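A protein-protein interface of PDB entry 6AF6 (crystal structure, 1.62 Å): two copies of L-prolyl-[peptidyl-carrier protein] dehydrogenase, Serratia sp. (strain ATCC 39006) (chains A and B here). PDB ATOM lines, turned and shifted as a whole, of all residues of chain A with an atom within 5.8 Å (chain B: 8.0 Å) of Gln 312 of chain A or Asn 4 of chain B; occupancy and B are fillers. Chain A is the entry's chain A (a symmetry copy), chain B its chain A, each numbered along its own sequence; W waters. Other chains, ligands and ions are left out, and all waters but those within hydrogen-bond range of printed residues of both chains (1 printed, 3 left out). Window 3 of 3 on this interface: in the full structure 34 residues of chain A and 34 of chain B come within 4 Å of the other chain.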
ATOM      1  N   MET A   1      24.822  13.354  11.736  1.00  0.00           N
ATOM      2  CA  MET A   1      23.464  13.729  11.333  1.00  0.00           C
ATOM      3  C   MET A   1      23.352  13.935   9.845  1.00  0.00           C
ATOM      4  O   MET A   1      24.032  14.782   9.282  1.00  0.00           O
ATOM      5  CB  MET A   1      23.035  14.996  12.063  1.00  0.00           C
ATOM      6  CG  MET A   1      21.578  15.390  11.870  1.00  0.00           C
ATOM      7  SD  MET A   1      20.398  14.442  12.850  1.00  0.00           S
ATOM      8  CE  MET A   1      21.021  14.688  14.507  1.00  0.00           C
ATOM      9  N   ASP A   2      22.456  13.179   9.216  1.00  0.00           N
ATOM     10  CA  ASP A   2      22.354  13.075   7.777  1.00  0.00           C
ATOM     11  C   ASP A   2      20.952  12.583   7.459  1.00  0.00           C
ATOM     12  O   ASP A   2      20.475  11.660   8.123  1.00  0.00           O
ATOM     13  CB  ASP A   2      23.404  12.047   7.259  1.00  0.00           C
ATOM     14  CG  ASP A   2      23.363  11.877   5.771  1.00  0.00           C
ATOM     15  OD1 ASP A   2      24.136  12.566   5.072  1.00  0.00           O
ATOM     16  OD2 ASP A   2      22.556  11.078   5.268  1.00  0.00           O
ATOM     17  N   TRP A 306      16.730   3.269  12.769  1.00  0.00           N
ATOM     18  CA  TRP A 306      18.166   3.507  12.786  1.00  0.00           C
ATOM     19  C   TRP A 306      18.747   3.219  14.174  1.00  0.00           C
ATOM     20  O   TRP A 306      19.811   2.582  14.281  1.00  0.00           O
ATOM     21  CB  TRP A 306      18.453   4.925  12.353  1.00  0.00           C
ATOM     22  CG  TRP A 306      19.929   5.296  12.404  1.00  0.00           C
ATOM     23  CD1 TRP A 306      20.854   5.136  11.388  1.00  0.00           C
ATOM     24  CD2 TRP A 306      20.616   5.926  13.478  1.00  0.00           C
ATOM     25  NE1 TRP A 306      22.069   5.650  11.779  1.00  0.00           N
ATOM     26  CE2 TRP A 306      21.955   6.109  13.065  1.00  0.00           C
ATOM     27  CE3 TRP A 306      20.239   6.323  14.763  1.00  0.00           C
ATOM     28  CZ2 TRP A 306      22.912   6.710  13.894  1.00  0.00           C
ATOM     29  CZ3 TRP A 306      21.198   6.937  15.575  1.00  0.00           C
ATOM     30  CH2 TRP A 306      22.508   7.104  15.134  1.00  0.00           C
ATOM     31  N   LYS A 307      18.076   3.675  15.252  1.00  0.00           N
ATOM     32  CA  LYS A 307      18.591   3.398  16.607  1.00  0.00           C
ATOM     33  C   LYS A 307      18.651   1.887  16.850  1.00  0.00           C
ATOM     34  O   LYS A 307      19.623   1.379  17.426  1.00  0.00           O
ATOM     35  CB  LYS A 307      17.734   4.065  17.692  1.00  0.00           C
ATOM     36  CG  LYS A 307      17.982   5.531  17.781  1.00  0.00           C
ATOM     37  CD  LYS A 307      16.950   6.128  18.723  1.00  0.00           C
ATOM     38  CE  LYS A 307      17.419   7.364  19.385  1.00  0.00           C
ATOM     39  NZ  LYS A 307      16.480   7.669  20.515  1.00  0.00           N
ATOM     40  N   HIS A 308      17.608   1.162  16.445  1.00  0.00           N
ATOM     41  CA  HIS A 308      17.647  -0.300  16.546  1.00  0.00           C
ATOM     42  C   HIS A 308      18.887  -0.869  15.854  1.00  0.00           C
ATOM     43  O   HIS A 308      19.633  -1.706  16.420  1.00  0.00           O
ATOM     44  CB  HIS A 308      16.385  -0.921  15.950  1.00  0.00           C
ATOM     45  CG  HIS A 308      16.348  -2.402  16.107  1.00  0.00           C
ATOM     46  ND1 HIS A 308      16.991  -3.255  15.234  1.00  0.00           N
ATOM     47  CD2 HIS A 308      15.778  -3.182  17.056  1.00  0.00           C
ATOM     48  CE1 HIS A 308      16.797  -4.501  15.627  1.00  0.00           C
ATOM     49  NE2 HIS A 308      16.061  -4.484  16.726  1.00  0.00           N
ATOM     50  N   ASP A 309      19.128  -0.436  14.627  1.00  0.00           N
ATOM     51  CA  ASP A 309      20.279  -0.910  13.853  1.00  0.00           C
ATOM     52  C   ASP A 309      21.586  -0.542  14.532  1.00  0.00           C
ATOM     53  O   ASP A 309      22.598  -1.216  14.304  1.00  0.00           O
ATOM     54  CB  ASP A 309      20.287  -0.356  12.440  1.00  0.00           C
ATOM     55  CG  ASP A 309      19.193  -0.966  11.568  1.00  0.00           C
ATOM     56  OD1 ASP A 309      18.710  -2.050  11.945  1.00  0.00           O
ATOM     57  OD2 ASP A 309      18.771  -0.337  10.564  1.00  0.00           O
ATOM     58  N   GLN A 310      21.614   0.550  15.311  1.00  0.00           N
ATOM     59  CA  GLN A 310      22.851   0.888  16.010  1.00  0.00           C
ATOM     60  C   GLN A 310      23.016   0.115  17.310  1.00  0.00           C
ATOM     61  O   GLN A 310      24.031   0.291  17.999  1.00  0.00           O
ATOM     62  CB  GLN A 310      22.921   2.404  16.293  1.00  0.00           C
ATOM     63  CG  GLN A 310      22.929   3.321  15.064  1.00  0.00           C
ATOM     64  CD  GLN A 310      24.292   3.405  14.405  1.00  0.00           C
ATOM     65  OE1 GLN A 310      24.445   3.156  13.202  1.00  0.00           O
ATOM     66  NE2 GLN A 310      25.294   3.789  15.187  1.00  0.00           N
ATOM     67  N   GLY A 311      22.059  -0.697  17.702  1.00  0.00           N
ATOM     68  CA  GLY A 311      22.114  -1.368  18.984  1.00  0.00           C
ATOM     69  C   GLY A 311      21.713  -0.521  20.167  1.00  0.00           C
ATOM     70  O   GLY A 311      21.946  -0.932  21.306  1.00  0.00           O
ATOM     71  N   GLN A 312      21.139   0.664  19.941  1.00  0.00           N
ATOM     72  CA  GLN A 312      20.599   1.482  21.021  1.00  0.00           C
ATOM     73  C   GLN A 312      19.237   0.937  21.446  1.00  0.00           C
ATOM     74  O   GLN A 312      18.641   0.085  20.773  1.00  0.00           O
ATOM     75  CB  GLN A 312      20.526   2.952  20.592  1.00  0.00           C
ATOM     76  CG  GLN A 312      21.875   3.517  20.243  1.00  0.00           C
ATOM     77  CD  GLN A 312      21.842   4.943  19.662  1.00  0.00           C
ATOM     78  OE1 GLN A 312      20.906   5.721  19.905  1.00  0.00           O
ATOM     79  NE2 GLN A 312      22.897   5.305  18.948  1.00  0.00           N
ATOM     80  N   ASP A 313      18.775   1.386  22.614  1.00  0.00           N
ATOM     81  CA  ASP A 313      17.456   1.025  23.130  1.00  0.00           C
ATOM     82  C   ASP A 313      16.421   1.784  22.314  1.00  0.00           C
ATOM     83  O   ASP A 313      16.359   3.015  22.394  1.00  0.00           O
ATOM     84  CB  ASP A 313      17.358   1.391  24.614  1.00  0.00           C
ATOM     85  CG  ASP A 313      16.035   0.931  25.271  1.00  0.00           C
ATOM     86  OD1 ASP A 313      15.222   0.204  24.639  1.00  0.00           O
ATOM     87  OD2 ASP A 313      15.819   1.304  26.448  1.00  0.00           O
ATOM     88  N   ALA A 314      15.663   1.080  21.478  1.00  0.00           N
ATOM     89  CA  ALA A 314      14.722   1.791  20.611  1.00  0.00           C
ATOM     90  C   ALA A 314      13.268   1.542  20.989  1.00  0.00           C
ATOM     91  O   ALA A 314      12.382   1.974  20.229  1.00  0.00           O
ATOM     92  CB  ALA A 314      14.930   1.420  19.146  1.00  0.00           C
ATOM     93  N   MET B   1      21.671   8.289   6.015  1.00  0.00           N
ATOM     94  CA  MET B   1      20.757   8.515   7.138  1.00  0.00           C
ATOM     95  C   MET B   1      21.388   8.171   8.461  1.00  0.00           C
ATOM     96  O   MET B   1      21.793   7.037   8.680  1.00  0.00           O
ATOM     97  CB  MET B   1      19.484   7.698   6.945  1.00  0.00           C
ATOM     98  CG  MET B   1      18.377   7.982   7.950  1.00  0.00           C
ATOM     99  SD  MET B   1      17.439   9.490   7.642  1.00  0.00           S
ATOM    100  CE  MET B   1      16.873   9.229   5.967  1.00  0.00           C
ATOM    101  N   ASP B   2      21.436   9.152   9.358  1.00  0.00           N
ATOM    102  CA  ASP B   2      22.189   9.084  10.591  1.00  0.00           C
ATOM    103  C   ASP B   2      21.590  10.104  11.543  1.00  0.00           C
ATOM    104  O   ASP B   2      21.309  11.228  11.118  1.00  0.00           O
ATOM    105  CB  ASP B   2      23.679   9.439  10.305  1.00  0.00           C
ATOM    106  CG  ASP B   2      24.531   9.394  11.536  1.00  0.00           C
ATOM    107  OD1 ASP B   2      25.147   8.338  11.795  1.00  0.00           O
ATOM    108  OD2 ASP B   2      24.593  10.391  12.275  1.00  0.00           O
ATOM    109  N   PHE B   3      21.456   9.754  12.822  1.00  0.00           N
ATOM    110  CA  PHE B   3      20.908  10.686  13.806  1.00  0.00           C
ATOM    111  C   PHE B   3      21.851  10.955  14.984  1.00  0.00           C
ATOM    112  O   PHE B   3      21.383  11.275  16.077  1.00  0.00           O
ATOM    113  CB  PHE B   3      19.548  10.178  14.301  1.00  0.00           C
ATOM    114  CG  PHE B   3      18.529  10.036  13.195  1.00  0.00           C
ATOM    115  CD1 PHE B   3      17.696  11.104  12.839  1.00  0.00           C
ATOM    116  CD2 PHE B   3      18.396   8.840  12.492  1.00  0.00           C
ATOM    117  CE1 PHE B   3      16.763  10.976  11.810  1.00  0.00           C
ATOM    118  CE2 PHE B   3      17.472   8.697  11.466  1.00  0.00           C
ATOM    119  CZ  PHE B   3      16.653   9.766  11.091  1.00  0.00           C
ATOM    120  N   ASN B   4      23.151  10.762  14.814  1.00  0.00           N
ATOM    121  CA  ASN B   4      24.106  11.122  15.855  1.00  0.00           C
ATOM    122  C   ASN B   4      24.743  12.446  15.458  1.00  0.00           C
ATOM    123  O   ASN B   4      24.865  12.779  14.273  1.00  0.00           O
ATOM    124  CB  ASN B   4      25.228  10.074  16.073  1.00  0.00           C
ATOM    125  CG  ASN B   4      24.825   8.818  16.943  1.00  0.00           C
ATOM    126  OD1 ASN B   4      24.045   8.856  17.939  1.00  0.00           O
ATOM    127  ND2 ASN B   4      25.442   7.687  16.569  1.00  0.00           N
ATOM    128  N   LEU B   5      25.134  13.205  16.467  1.00  0.00           N
ATOM    129  CA  LEU B   5      25.943  14.388  16.256  1.00  0.00           C
ATOM    130  C   LEU B   5      27.401  13.965  16.070  1.00  0.00           C
ATOM    131  O   LEU B   5      27.868  13.016  16.721  1.00  0.00           O
ATOM    132  CB  LEU B   5      25.809  15.288  17.475  1.00  0.00           C
ATOM    133  CG  LEU B   5      24.421  15.836  17.811  1.00  0.00           C
ATOM    134  CD1 LEU B   5      24.559  16.822  18.953  1.00  0.00           C
ATOM    135  CD2 LEU B   5      23.849  16.487  16.595  1.00  0.00           C
ATOM    136  N   SER B   6      28.104  14.678  15.202  1.00  0.00           N
ATOM    137  CA  SER B   6      29.550  14.581  15.158  1.00  0.00           C
ATOM    138  C   SER B   6      30.150  15.041  16.481  1.00  0.00           C
ATOM    139  O   SER B   6      29.483  15.693  17.312  1.00  0.00           O
ATOM    140  CB  SER B   6      30.082  15.427  14.024  1.00  0.00           C
ATOM    141  OG  SER B   6      30.052  16.799  14.353  1.00  0.00           O
ATOM    142  N   ASN B   7      31.423  14.679  16.706  1.00  0.00           N
ATOM    143  CA  ASN B   7      32.078  15.145  17.931  1.00  0.00           C
ATOM    144  C   ASN B   7      32.154  16.666  17.946  1.00  0.00           C
ATOM    145  O   ASN B   7      31.988  17.303  18.996  1.00  0.00           O
ATOM    146  CB  ASN B   7      33.474  14.530  18.044  1.00  0.00           C
ATOM    147  CG  ASN B   7      33.423  13.044  18.292  1.00  0.00           C
ATOM    148  OD1 ASN B   7      32.590  12.556  19.073  1.00  0.00           O
ATOM    149  ND2 ASN B   7      34.303  12.300  17.622  1.00  0.00           N
ATOM    150  N   GLN B   9      29.948  18.724  16.487  1.00  0.00           N
ATOM    151  CA  GLN B   9      28.607  19.210  16.827  1.00  0.00           C
ATOM    152  C   GLN B   9      28.309  19.057  18.303  1.00  0.00           C
ATOM    153  O   GLN B   9      27.740  19.966  18.940  1.00  0.00           O
ATOM    154  CB  GLN B   9      27.573  18.442  16.008  1.00  0.00           C
ATOM    155  CG  GLN B   9      27.584  18.901  14.577  1.00  0.00           C
ATOM    156  CD  GLN B   9      26.857  17.962  13.643  1.00  0.00           C
ATOM    157  OE1 GLN B   9      26.736  16.756  13.881  1.00  0.00           O
ATOM    158  NE2 GLN B   9      26.311  18.531  12.583  1.00  0.00           N
ATOM    159  N   SER B  10      28.665  17.913  18.880  1.00  0.00           N
ATOM    160  CA  SER B  10      28.468  17.716  20.310  1.00  0.00           C
ATOM    161  C   SER B  10      29.227  18.756  21.129  1.00  0.00           C
ATOM    162  O   SER B  10      28.710  19.290  22.121  1.00  0.00           O
ATOM    163  CB  SER B  10      28.940  16.315  20.710  1.00  0.00           C
ATOM    164  OG  SER B  10      28.109  15.327  20.168  1.00  0.00           O
ATOM    165  N   LEU B  67      22.958  24.055  10.714  1.00  0.00           N
ATOM    166  CA  LEU B  67      22.706  23.067  11.768  1.00  0.00           C
ATOM    167  C   LEU B  67      23.548  23.362  13.005  1.00  0.00           C
ATOM    168  O   LEU B  67      23.033  23.312  14.128  1.00  0.00           O
ATOM    169  CB  LEU B  67      22.914  21.638  11.261  1.00  0.00           C
ATOM    170  CG  LEU B  67      22.696  20.523  12.292  1.00  0.00           C
ATOM    171  CD1 LEU B  67      21.233  20.628  12.849  1.00  0.00           C
ATOM    172  CD2 LEU B  67      22.894  19.171  11.629  1.00  0.00           C
HETATM  173  O   HOH W   1      26.915  15.063  11.321  1.00  0.00           O
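The backbone NH (N) of Asn 4 of chain B sits at hydrogen-bond distance from the side-chain carboxylate (OD2) of Asp 2 of chain B. O of Lys 307 of chain A sits at hydrogen-bond distance from N of Gln 312 of chain A (3.0 Å).
Met 1 of chain A touches Asp 2 of chain B, and with the chains exchanged Asp 2 of chain A touches Met 1 of chain B. Asp 2 of chain B touches its own counterpart, Asp 2 of chain A. Of the 11 pairs that touch across the chains among the printed residues, 3 have their exchanged pair printed and touching as well.
Water W1 lies within hydrogen-bond range of N of Met 1 of chain A (2.7 Å) and OE1 of Gln 9 of chain B (3.1 Å).
Of the printed residues of chain B, Met 1 of chain A touches Asp 2 (3.0 Å), Phe 3 (3.8 Å), Asn 4 (2.6 Å) and Leu 5 (3.9 Å). Of the printed residues of chain B, Asp 2 of chain A touches Met 1 (3.0 Å) and Asp 2 (3.0 Å). Gln 310 of chain A touches none of the printed residues of chain B. No residue of chain B comes within 4 Å of Gly 311 of chain A. Gln 312 of chain A touches just one residue of chain B: Asn 4. Of the printed residues of chain A, Met 1 of chain B touches Asp 2 and Trp 306. Printed residues of chain A within 4 Å of Asn 4 of chain B: Met 1 (2.6 Å), Trp 306 (3.3 Å) and Gln 312 (3.9 Å). Printed residues of chain A within 4 Å of Leu 5 of chain B: Met 1 (3.9 Å). Asn 7 of chain B touches none of the printed residues of chain A. The nearest printed residue of chain A that does not touch Asn 4 of chain B is Gln 310 of chain A (4.1 Å).
Hydrophobic or aromatic side chains of chain B that line the printed part of chain A: Met 1, Phe 3 and Leu 5. Among the printed residues, 11 pairs touch across the chains.
Among the printed residues, pairs that only touch across the chains: Met 1 of chain A with Phe 3 of chain B (3.8 Å), Met 1 of chain A with Leu 5 of chain B (3.9 Å), Trp 306 of chain A with Asp 2 of chain B (3.5 Å), Trp 306 of chain A with Phe 3 of chain B (3.5 Å), Trp 306 of chain A with Asn 4 of chain B (3.3 Å) and Gln 312 of chain A with Asn 4 of chain B (3.9 Å).
The backbone carbonyl oxygen (O) of Asn 4 of chain B sits at hydrogen-bond distance from the backbone NH (N) of Met 1 of chain A (2.6 Å). The backbone NH (N) of Met 1 of chain B sits at hydrogen-bond distance from the side-chain carboxylate (OD2) of Asp 2 of chain A (3.0 Å). OD2 of Asp 2 of chain B sits at hydrogen-bond distance from N of Met 1 of chain A (3.0 Å). The indole nitrogen (NE1) of Trp 306 of chain A sits at hydrogen-bond distance from the backbone carbonyl oxygen (O) of Met 1 of chain B. The backbone NH (N) of Asp 2 of chain B sits at hydrogen-bond distance from the backbone carbonyl oxygen (O) of Asp 2 of chain A.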
